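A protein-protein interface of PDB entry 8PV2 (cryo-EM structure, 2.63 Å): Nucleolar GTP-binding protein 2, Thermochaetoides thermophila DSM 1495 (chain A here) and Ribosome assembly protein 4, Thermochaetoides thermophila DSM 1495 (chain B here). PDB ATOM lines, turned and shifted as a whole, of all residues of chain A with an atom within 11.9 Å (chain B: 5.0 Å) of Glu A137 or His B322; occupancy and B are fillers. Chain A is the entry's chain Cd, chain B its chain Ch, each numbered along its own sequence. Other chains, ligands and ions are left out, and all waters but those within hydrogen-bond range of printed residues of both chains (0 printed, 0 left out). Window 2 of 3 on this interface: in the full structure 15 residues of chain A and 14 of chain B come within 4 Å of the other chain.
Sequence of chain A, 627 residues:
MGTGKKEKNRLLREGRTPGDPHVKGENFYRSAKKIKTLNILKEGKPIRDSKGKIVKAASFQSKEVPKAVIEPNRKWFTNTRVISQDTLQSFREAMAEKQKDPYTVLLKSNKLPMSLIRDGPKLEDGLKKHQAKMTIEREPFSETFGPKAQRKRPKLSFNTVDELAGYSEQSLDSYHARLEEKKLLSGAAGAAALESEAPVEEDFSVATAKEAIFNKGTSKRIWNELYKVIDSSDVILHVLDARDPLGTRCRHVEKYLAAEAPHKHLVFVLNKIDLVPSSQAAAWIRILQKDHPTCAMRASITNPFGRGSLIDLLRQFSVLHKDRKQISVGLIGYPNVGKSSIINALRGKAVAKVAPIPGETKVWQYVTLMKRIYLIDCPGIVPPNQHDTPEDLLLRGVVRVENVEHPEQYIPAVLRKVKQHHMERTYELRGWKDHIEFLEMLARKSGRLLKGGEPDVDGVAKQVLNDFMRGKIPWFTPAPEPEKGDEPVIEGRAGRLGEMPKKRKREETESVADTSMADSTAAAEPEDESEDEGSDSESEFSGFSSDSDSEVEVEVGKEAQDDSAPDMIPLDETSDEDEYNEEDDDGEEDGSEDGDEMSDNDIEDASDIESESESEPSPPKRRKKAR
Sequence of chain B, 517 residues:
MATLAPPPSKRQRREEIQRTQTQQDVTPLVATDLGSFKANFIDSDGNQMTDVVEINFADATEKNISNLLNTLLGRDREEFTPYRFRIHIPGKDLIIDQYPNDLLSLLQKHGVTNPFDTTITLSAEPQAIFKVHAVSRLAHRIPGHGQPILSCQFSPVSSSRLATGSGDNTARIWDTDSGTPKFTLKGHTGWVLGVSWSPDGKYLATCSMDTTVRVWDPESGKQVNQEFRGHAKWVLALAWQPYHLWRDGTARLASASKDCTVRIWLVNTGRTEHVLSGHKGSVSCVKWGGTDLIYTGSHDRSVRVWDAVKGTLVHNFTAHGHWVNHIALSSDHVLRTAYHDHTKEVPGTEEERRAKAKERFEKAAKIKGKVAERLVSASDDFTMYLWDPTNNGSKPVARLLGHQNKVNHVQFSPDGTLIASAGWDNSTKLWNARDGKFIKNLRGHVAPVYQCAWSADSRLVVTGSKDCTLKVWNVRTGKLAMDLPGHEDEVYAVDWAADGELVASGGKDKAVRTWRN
The backbone carbonyl oxygen (O) of Trp B323 is in hydrogen-bond range of the backbone NH (N) of Asp B380 (2.9 Å). The backbone carbonyl oxygen of His B322 sits at hydrogen-bond distance from the side-chain hydroxyl of Ser B379. OG of Ser B379 sits close to N of Asp B381, at 3.3 Å. The side-chain carboxylate (OE1) of Glu A139 lies within salt-bridge range of the guanidinium group (NH1) of Arg A138, 3.2 Å away. OD2 of Asp B381 sits close to ND1 of His B320. OD2 of Asp B381 is in hydrogen-bond range of N of Gly B321.
The backbone carbonyl oxygen of Gly B321 sits at hydrogen-bond distance from the guanidinium group of Arg A138, 3.1 Å away. The side-chain carboxylate (OE1) of Glu A137 lies within hydrogen-bond range of a ring nitrogen (NE2) of His B322, at 2.9 Å.
Met A134 touches Asp B380. Asp B381 touches Met A134 (CA to CE, 3.7 Å). CG of Arg A138 touches NH1 of Arg B301, 3.7 Å away.
Hydrophobic or aromatic side chains of chain A within 4 Å of the printed part of chain B: Met A134. Of the 9 printed residues of chain B, 5 touch a printed residue of chain A. Hydrophobic or aromatic side chains of chain B that line the printed part of chain A: His B322. Among the printed residues, 5 pairs touch across the chains. Among the printed residues, no Asp or Glu carboxylate lies within 4 Å of a Lys or Arg side-chain nitrogen of the other chain.
Of the printed residues of chain B, Glu A137 touches His B322. His B322 touches one residue of chain A. No residue of chain A comes within 4 Å of His B320. No residue of chain A comes within 4 Å of Trp B323. No residue of chain A comes within 4 Å of Ser B379. Asp B380 touches one residue of chain A. Of the printed residues of chain B, Arg A138 touches Arg B301 (3.7 Å) and Gly B321 (3.1 Å). Printed residues of chain B within 4 Å of Met A134: Asp B380 (3.8 Å) and Asp B381 (3.7 Å). The nearest residue of chain A that does not touch His B322 is Met A134 (4.2 Å).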
ATOM      1  N   LEU A 127      18.134  27.610 -39.461  1.00  0.00           N
ATOM      2  CA  LEU A 127      18.168  27.601 -38.001  1.00  0.00           C
ATOM      3  C   LEU A 127      17.288  28.692 -37.396  1.00  0.00           C
ATOM      4  O   LEU A 127      16.580  28.442 -36.410  1.00  0.00           O
ATOM      5  CB  LEU A 127      19.604  27.742 -37.503  1.00  0.00           C
ATOM      6  CG  LEU A 127      20.524  26.571 -37.831  1.00  0.00           C
ATOM      7  CD1 LEU A 127      21.949  26.879 -37.413  1.00  0.00           C
ATOM      8  CD2 LEU A 127      20.023  25.318 -37.140  1.00  0.00           C
ATOM      9  N   LYS A 129      14.648  30.225 -38.548  1.00  0.00           N
ATOM     10  CA  LYS A 129      13.203  30.081 -38.697  1.00  0.00           C
ATOM     11  C   LYS A 129      12.612  29.136 -37.664  1.00  0.00           C
ATOM     12  O   LYS A 129      11.389  29.105 -37.499  1.00  0.00           O
ATOM     13  CB  LYS A 129      12.813  29.593 -40.097  1.00  0.00           C
ATOM     14  CG  LYS A 129      13.203  30.470 -41.297  1.00  0.00           C
ATOM     15  CD  LYS A 129      12.438  31.789 -41.440  1.00  0.00           C
ATOM     16  CE  LYS A 129      13.171  32.962 -40.789  1.00  0.00           C
ATOM     17  NZ  LYS A 129      12.494  34.261 -41.015  1.00  0.00           N
ATOM     18  N   HIS A 130      13.443  28.367 -36.968  1.00  0.00           N
ATOM     19  CA  HIS A 130      12.962  27.420 -35.979  1.00  0.00           C
ATOM     20  C   HIS A 130      13.517  27.658 -34.586  1.00  0.00           C
ATOM     21  O   HIS A 130      13.164  26.903 -33.673  1.00  0.00           O
ATOM     22  CB  HIS A 130      13.286  25.991 -36.424  1.00  0.00           C
ATOM     23  CG  HIS A 130      12.785  25.668 -37.794  1.00  0.00           C
ATOM     24  ND1 HIS A 130      13.600  25.668 -38.905  1.00  0.00           N
ATOM     25  CD2 HIS A 130      11.548  25.341 -38.236  1.00  0.00           C
ATOM     26  CE1 HIS A 130      12.888  25.353 -39.972  1.00  0.00           C
ATOM     27  NE2 HIS A 130      11.639  25.149 -39.593  1.00  0.00           N
ATOM     28  N   GLN A 131      14.380  28.665 -34.404  1.00  0.00           N
ATOM     29  CA  GLN A 131      14.883  28.990 -33.068  1.00  0.00           C
ATOM     30  C   GLN A 131      13.759  29.298 -32.085  1.00  0.00           C
ATOM     31  O   GLN A 131      13.796  28.842 -30.938  1.00  0.00           O
ATOM     32  CB  GLN A 131      15.847  30.172 -33.134  1.00  0.00           C
ATOM     33  CG  GLN A 131      17.260  29.805 -33.522  1.00  0.00           C
ATOM     34  CD  GLN A 131      17.915  28.896 -32.511  1.00  0.00           C
ATOM     35  OE1 GLN A 131      18.134  27.712 -32.770  1.00  0.00           O
ATOM     36  NE2 GLN A 131      18.231  29.442 -31.344  1.00  0.00           N
ATOM     37  N   ALA A 132      12.749  30.059 -32.514  1.00  0.00           N
ATOM     38  CA  ALA A 132      11.677  30.456 -31.604  1.00  0.00           C
ATOM     39  C   ALA A 132      10.852  29.256 -31.152  1.00  0.00           C
ATOM     40  O   ALA A 132      10.605  29.067 -29.953  1.00  0.00           O
ATOM     41  CB  ALA A 132      10.787  31.497 -32.278  1.00  0.00           C
ATOM     42  N   LYS A 133      10.444  28.417 -32.106  1.00  0.00           N
ATOM     43  CA  LYS A 133       9.662  27.230 -31.785  1.00  0.00           C
ATOM     44  C   LYS A 133      10.477  26.252 -30.956  1.00  0.00           C
ATOM     45  O   LYS A 133       9.946  25.595 -30.058  1.00  0.00           O
ATOM     46  CB  LYS A 133       9.173  26.553 -33.067  1.00  0.00           C
ATOM     47  CG  LYS A 133       7.919  27.167 -33.684  1.00  0.00           C
ATOM     48  CD  LYS A 133       8.237  28.437 -34.468  1.00  0.00           C
ATOM     49  CE  LYS A 133       7.004  29.047 -35.106  1.00  0.00           C
ATOM     50  NZ  LYS A 133       7.333  30.354 -35.743  1.00  0.00           N
ATOM     51  N   MET A 134      11.777  26.164 -31.234  1.00  0.00           N
ATOM     52  CA  MET A 134      12.652  25.259 -30.505  1.00  0.00           C
ATOM     53  C   MET A 134      12.820  25.702 -29.057  1.00  0.00           C
ATOM     54  O   MET A 134      12.791  24.870 -28.142  1.00  0.00           O
ATOM     55  CB  MET A 134      13.992  25.206 -31.226  1.00  0.00           C
ATOM     56  CG  MET A 134      14.999  24.227 -30.711  1.00  0.00           C
ATOM     57  SD  MET A 134      16.437  24.412 -31.769  1.00  0.00           S
ATOM     58  CE  MET A 134      15.810  23.677 -33.276  1.00  0.00           C
ATOM     59  N   THR A 135      12.978  27.012 -28.832  1.00  0.00           N
ATOM     60  CA  THR A 135      13.064  27.528 -27.468  1.00  0.00           C
ATOM     61  C   THR A 135      11.764  27.312 -26.708  1.00  0.00           C
ATOM     62  O   THR A 135      11.785  26.992 -25.515  1.00  0.00           O
ATOM     63  CB  THR A 135      13.423  29.015 -27.467  1.00  0.00           C
ATOM     64  OG1 THR A 135      12.544  29.728 -28.341  1.00  0.00           O
ATOM     65  CG2 THR A 135      14.859  29.227 -27.907  1.00  0.00           C
ATOM     66  N   ILE A 136      10.621  27.492 -27.375  1.00  0.00           N
ATOM     67  CA  ILE A 136       9.352  27.274 -26.683  1.00  0.00           C
ATOM     68  C   ILE A 136       9.129  25.792 -26.380  1.00  0.00           C
ATOM     69  O   ILE A 136       8.591  25.448 -25.319  1.00  0.00           O
ATOM     70  CB  ILE A 136       8.192  27.890 -27.486  1.00  0.00           C
ATOM     71  CG1 ILE A 136       8.408  29.393 -27.626  1.00  0.00           C
ATOM     72  CG2 ILE A 136       6.867  27.668 -26.797  1.00  0.00           C
ATOM     73  CD1 ILE A 136       8.700  30.098 -26.315  1.00  0.00           C
ATOM     74  N   GLU A 137       9.538  24.889 -27.279  1.00  0.00           N
ATOM     75  CA  GLU A 137       9.448  23.461 -26.977  1.00  0.00           C
ATOM     76  C   GLU A 137      10.360  23.068 -25.824  1.00  0.00           C
ATOM     77  O   GLU A 137       9.993  22.224 -25.001  1.00  0.00           O
ATOM     78  CB  GLU A 137       9.776  22.614 -28.205  1.00  0.00           C
ATOM     79  CG  GLU A 137       8.774  22.702 -29.331  1.00  0.00           C
ATOM     80  CD  GLU A 137       9.172  21.853 -30.521  1.00  0.00           C
ATOM     81  OE1 GLU A 137      10.290  21.298 -30.511  1.00  0.00           O
ATOM     82  OE2 GLU A 137       8.363  21.733 -31.464  1.00  0.00           O
ATOM     83  N   ARG A 138      11.559  23.650 -25.760  1.00  0.00           N
ATOM     84  CA  ARG A 138      12.455  23.361 -24.647  1.00  0.00           C
ATOM     85  C   ARG A 138      11.894  23.880 -23.330  1.00  0.00           C
ATOM     86  O   ARG A 138      11.868  23.154 -22.332  1.00  0.00           O
ATOM     87  CB  ARG A 138      13.831  23.962 -24.916  1.00  0.00           C
ATOM     88  CG  ARG A 138      14.871  23.630 -23.866  1.00  0.00           C
ATOM     89  CD  ARG A 138      16.106  24.517 -23.976  1.00  0.00           C
ATOM     90  NE  ARG A 138      16.519  24.746 -25.355  1.00  0.00           N
ATOM     91  CZ  ARG A 138      16.457  25.918 -25.972  1.00  0.00           C
ATOM     92  NH1 ARG A 138      16.014  27.001 -25.355  1.00  0.00           N
ATOM     93  NH2 ARG A 138      16.850  26.006 -27.238  1.00  0.00           N
ATOM     94  N   GLU A 139      11.443  25.132 -23.306  1.00  0.00           N
ATOM     95  CA  GLU A 139      10.888  25.750 -22.104  1.00  0.00           C
ATOM     96  C   GLU A 139       9.542  26.370 -22.453  1.00  0.00           C
ATOM     97  O   GLU A 139       9.490  27.342 -23.225  1.00  0.00           O
ATOM     98  CB  GLU A 139      11.834  26.805 -21.547  1.00  0.00           C
ATOM     99  CG  GLU A 139      13.270  26.350 -21.393  1.00  0.00           C
ATOM    100  CD  GLU A 139      14.257  27.493 -21.481  1.00  0.00           C
ATOM    101  OE1 GLU A 139      15.227  27.379 -22.257  1.00  0.00           O
ATOM    102  OE2 GLU A 139      14.066  28.506 -20.777  1.00  0.00           O
ATOM    103  N   PRO A 140       8.440  25.840 -21.929  1.00  0.00           N
ATOM    104  CA  PRO A 140       7.139  26.475 -22.161  1.00  0.00           C
ATOM    105  C   PRO A 140       7.021  27.809 -21.438  1.00  0.00           C
ATOM    106  O   PRO A 140       7.802  28.124 -20.539  1.00  0.00           O
ATOM    107  CB  PRO A 140       6.134  25.453 -21.617  1.00  0.00           C
ATOM    108  CG  PRO A 140       6.921  24.475 -20.843  1.00  0.00           C
ATOM    109  CD  PRO A 140       8.309  24.489 -21.363  1.00  0.00           C
ATOM    110  N   PHE A 141       6.035  28.606 -21.861  1.00  0.00           N
ATOM    111  CA  PHE A 141       5.830  29.929 -21.276  1.00  0.00           C
ATOM    112  C   PHE A 141       5.417  29.836 -19.813  1.00  0.00           C
ATOM    113  O   PHE A 141       5.748  30.714 -19.008  1.00  0.00           O
ATOM    114  CB  PHE A 141       4.774  30.701 -22.064  1.00  0.00           C
ATOM    115  CG  PHE A 141       5.299  31.372 -23.294  1.00  0.00           C
ATOM    116  CD1 PHE A 141       6.238  32.381 -23.200  1.00  0.00           C
ATOM    117  CD2 PHE A 141       4.839  31.005 -24.546  1.00  0.00           C
ATOM    118  CE1 PHE A 141       6.719  33.001 -24.330  1.00  0.00           C
ATOM    119  CE2 PHE A 141       5.316  31.625 -25.678  1.00  0.00           C
ATOM    120  CZ  PHE A 141       6.255  32.625 -25.570  1.00  0.00           C
ATOM    121  N   SER A 142       4.683  28.785 -19.451  1.00  0.00           N
ATOM    122  CA  SER A 142       4.198  28.644 -18.087  1.00  0.00           C
ATOM    123  C   SER A 142       5.297  28.257 -17.108  1.00  0.00           C
ATOM    124  O   SER A 142       5.185  28.576 -15.922  1.00  0.00           O
ATOM    125  CB  SER A 142       3.071  27.618 -18.041  1.00  0.00           C
ATOM    126  OG  SER A 142       3.506  26.367 -18.534  1.00  0.00           O
ATOM    127  N   GLU A 143       6.342  27.572 -17.565  1.00  0.00           N
ATOM    128  CA  GLU A 143       7.455  27.206 -16.701  1.00  0.00           C
ATOM    129  C   GLU A 143       8.493  28.305 -16.558  1.00  0.00           C
ATOM    130  O   GLU A 143       9.360  28.202 -15.686  1.00  0.00           O
ATOM    131  CB  GLU A 143       8.149  25.947 -17.219  1.00  0.00           C
ATOM    132  CG  GLU A 143       7.333  24.684 -17.109  1.00  0.00           C
ATOM    133  CD  GLU A 143       8.073  23.482 -17.648  1.00  0.00           C
ATOM    134  OE1 GLU A 143       9.174  23.668 -18.204  1.00  0.00           O
ATOM    135  OE2 GLU A 143       7.561  22.352 -17.510  1.00  0.00           O
ATOM    136  N   THR A 144       8.435  29.345 -17.382  1.00  0.00           N
ATOM    137  CA  THR A 144       9.425  30.411 -17.339  1.00  0.00           C
ATOM    138  C   THR A 144       9.041  31.503 -16.350  1.00  0.00           C
ATOM    139  O   THR A 144       9.800  31.802 -15.424  1.00  0.00           O
ATOM    140  CB  THR A 144       9.616  31.005 -18.734  1.00  0.00           C
ATOM    141  OG1 THR A 144      10.133  30.001 -19.614  1.00  0.00           O
ATOM    142  CG2 THR A 144      10.571  32.169 -18.688  1.00  0.00           C
ATOM    143  N   ARG B 301      18.293  16.610 -23.130  1.00  0.00           N
ATOM    144  CA  ARG B 301      19.251  17.361 -23.938  1.00  0.00           C
ATOM    145  C   ARG B 301      20.687  17.137 -23.487  1.00  0.00           C
ATOM    146  O   ARG B 301      21.521  18.030 -23.665  1.00  0.00           O
ATOM    147  CB  ARG B 301      18.947  18.864 -23.934  1.00  0.00           C
ATOM    148  CG  ARG B 301      17.510  19.192 -24.264  1.00  0.00           C
ATOM    149  CD  ARG B 301      17.241  20.662 -24.140  1.00  0.00           C
ATOM    150  NE  ARG B 301      17.589  21.150 -22.813  1.00  0.00           N
ATOM    151  CZ  ARG B 301      16.776  21.111 -21.767  1.00  0.00           C
ATOM    152  NH1 ARG B 301      15.555  20.609 -21.859  1.00  0.00           N
ATOM    153  NH2 ARG B 301      17.197  21.588 -20.601  1.00  0.00           N
ATOM    154  N   HIS B 320      23.585  20.387 -26.385  1.00  0.00           N
ATOM    155  CA  HIS B 320      22.462  20.334 -27.313  1.00  0.00           C
ATOM    156  C   HIS B 320      21.272  21.122 -26.784  1.00  0.00           C
ATOM    157  O   HIS B 320      21.087  21.265 -25.573  1.00  0.00           O
ATOM    158  CB  HIS B 320      22.048  18.888 -27.574  1.00  0.00           C
ATOM    159  CG  HIS B 320      22.967  18.147 -28.494  1.00  0.00           C
ATOM    160  ND1 HIS B 320      23.107  18.471 -29.825  1.00  0.00           N
ATOM    161  CD2 HIS B 320      23.776  17.085 -28.279  1.00  0.00           C
ATOM    162  CE1 HIS B 320      23.964  17.641 -30.390  1.00  0.00           C
ATOM    163  NE2 HIS B 320      24.391  16.797 -29.472  1.00  0.00           N
ATOM    164  N   GLY B 321      20.465  21.637 -27.703  1.00  0.00           N
ATOM    165  CA  GLY B 321      19.300  22.431 -27.387  1.00  0.00           C
ATOM    166  C   GLY B 321      17.968  21.719 -27.469  1.00  0.00           C
ATOM    167  O   GLY B 321      16.936  22.362 -27.263  1.00  0.00           O
ATOM    168  N   HIS B 322      17.948  20.428 -27.779  1.00  0.00           N
ATOM    169  CA  HIS B 322      16.713  19.655 -27.814  1.00  0.00           C
ATOM    170  C   HIS B 322      17.084  18.190 -27.598  1.00  0.00           C
ATOM    171  O   HIS B 322      18.195  17.881 -27.158  1.00  0.00           O
ATOM    172  CB  HIS B 322      15.949  19.888 -29.120  1.00  0.00           C
ATOM    173  CG  HIS B 322      14.461  19.814 -28.973  1.00  0.00           C
ATOM    174  ND1 HIS B 322      13.754  18.637 -29.072  1.00  0.00           N
ATOM    175  CD2 HIS B 322      13.543  20.782 -28.746  1.00  0.00           C
ATOM    176  CE1 HIS B 322      12.467  18.880 -28.906  1.00  0.00           C
ATOM    177  NE2 HIS B 322      12.312  20.174 -28.705  1.00  0.00           N
ATOM    178  N   TRP B 323      16.143  17.293 -27.899  1.00  0.00           N
ATOM    179  CA  TRP B 323      16.302  15.860 -27.670  1.00  0.00           C
ATOM    180  C   TRP B 323      17.518  15.306 -28.395  1.00  0.00           C
ATOM    181  O   TRP B 323      17.706  15.534 -29.590  1.00  0.00           O
ATOM    182  CB  TRP B 323      15.071  15.105 -28.170  1.00  0.00           C
ATOM    183  CG  TRP B 323      13.836  15.270 -27.376  1.00  0.00           C
ATOM    184  CD1 TRP B 323      13.656  16.047 -26.277  1.00  0.00           C
ATOM    185  CD2 TRP B 323      12.592  14.614 -27.614  1.00  0.00           C
ATOM    186  NE1 TRP B 323      12.371  15.922 -25.817  1.00  0.00           N
ATOM    187  CE2 TRP B 323      11.698  15.045 -26.622  1.00  0.00           C
ATOM    188  CE3 TRP B 323      12.146  13.702 -28.574  1.00  0.00           C
ATOM    189  CZ2 TRP B 323      10.385  14.597 -26.561  1.00  0.00           C
ATOM    190  CZ3 TRP B 323      10.848  13.258 -28.512  1.00  0.00           C
ATOM    191  CH2 TRP B 323       9.979  13.705 -27.514  1.00  0.00           C
ATOM    192  N   VAL B 324      18.333  14.546 -27.673  1.00  0.00           N
ATOM    193  CA  VAL B 324      19.459  13.842 -28.272  1.00  0.00           C
ATOM    194  C   VAL B 324      18.963  12.490 -28.761  1.00  0.00           C
ATOM    195  O   VAL B 324      18.729  11.576 -27.964  1.00  0.00           O
ATOM    196  CB  VAL B 324      20.614  13.682 -27.272  1.00  0.00           C
ATOM    197  CG1 VAL B 324      21.750  12.902 -27.902  1.00  0.00           C
ATOM    198  CG2 VAL B 324      21.095  15.035 -26.800  1.00  0.00           C
ATOM    199  N   SER B 379      21.085  15.603 -32.661  1.00  0.00           N
ATOM    200  CA  SER B 379      19.935  16.036 -31.882  1.00  0.00           C
ATOM    201  C   SER B 379      18.858  16.654 -32.754  1.00  0.00           C
ATOM    202  O   SER B 379      19.024  16.839 -33.961  1.00  0.00           O
ATOM    203  CB  SER B 379      20.326  17.036 -30.796  1.00  0.00           C
ATOM    204  OG  SER B 379      19.176  17.538 -30.144  1.00  0.00           O
ATOM    205  N   ASP B 380      17.737  16.976 -32.101  1.00  0.00           N
ATOM    206  CA  ASP B 380      16.585  17.692 -32.633  1.00  0.00           C
ATOM    207  C   ASP B 380      16.827  19.152 -32.761  1.00  0.00           C
ATOM    208  O   ASP B 380      15.965  19.833 -33.317  1.00  0.00           O
ATOM    209  CB  ASP B 380      15.354  17.474 -31.757  1.00  0.00           C
ATOM    210  CG  ASP B 380      14.670  16.170 -32.029  1.00  0.00           C
ATOM    211  OD1 ASP B 380      15.159  15.408 -32.884  1.00  0.00           O
ATOM    212  OD2 ASP B 380      13.625  15.912 -31.402  1.00  0.00           O
ATOM    213  N   ASP B 381      17.948  19.690 -32.287  1.00  0.00           N
ATOM    214  CA  ASP B 381      18.304  21.076 -32.554  1.00  0.00           C
ATOM    215  C   ASP B 381      18.964  21.259 -33.914  1.00  0.00           C
ATOM    216  O   ASP B 381      19.667  22.251 -34.117  1.00  0.00           O
ATOM    217  CB  ASP B 381      19.200  21.633 -31.440  1.00  0.00           C
ATOM    218  CG  ASP B 381      20.484  20.847 -31.242  1.00  0.00           C
ATOM    219  OD1 ASP B 381      20.820  19.962 -32.047  1.00  0.00           O
ATOM    220  OD2 ASP B 381      21.183  21.137 -30.256  1.00  0.00           O
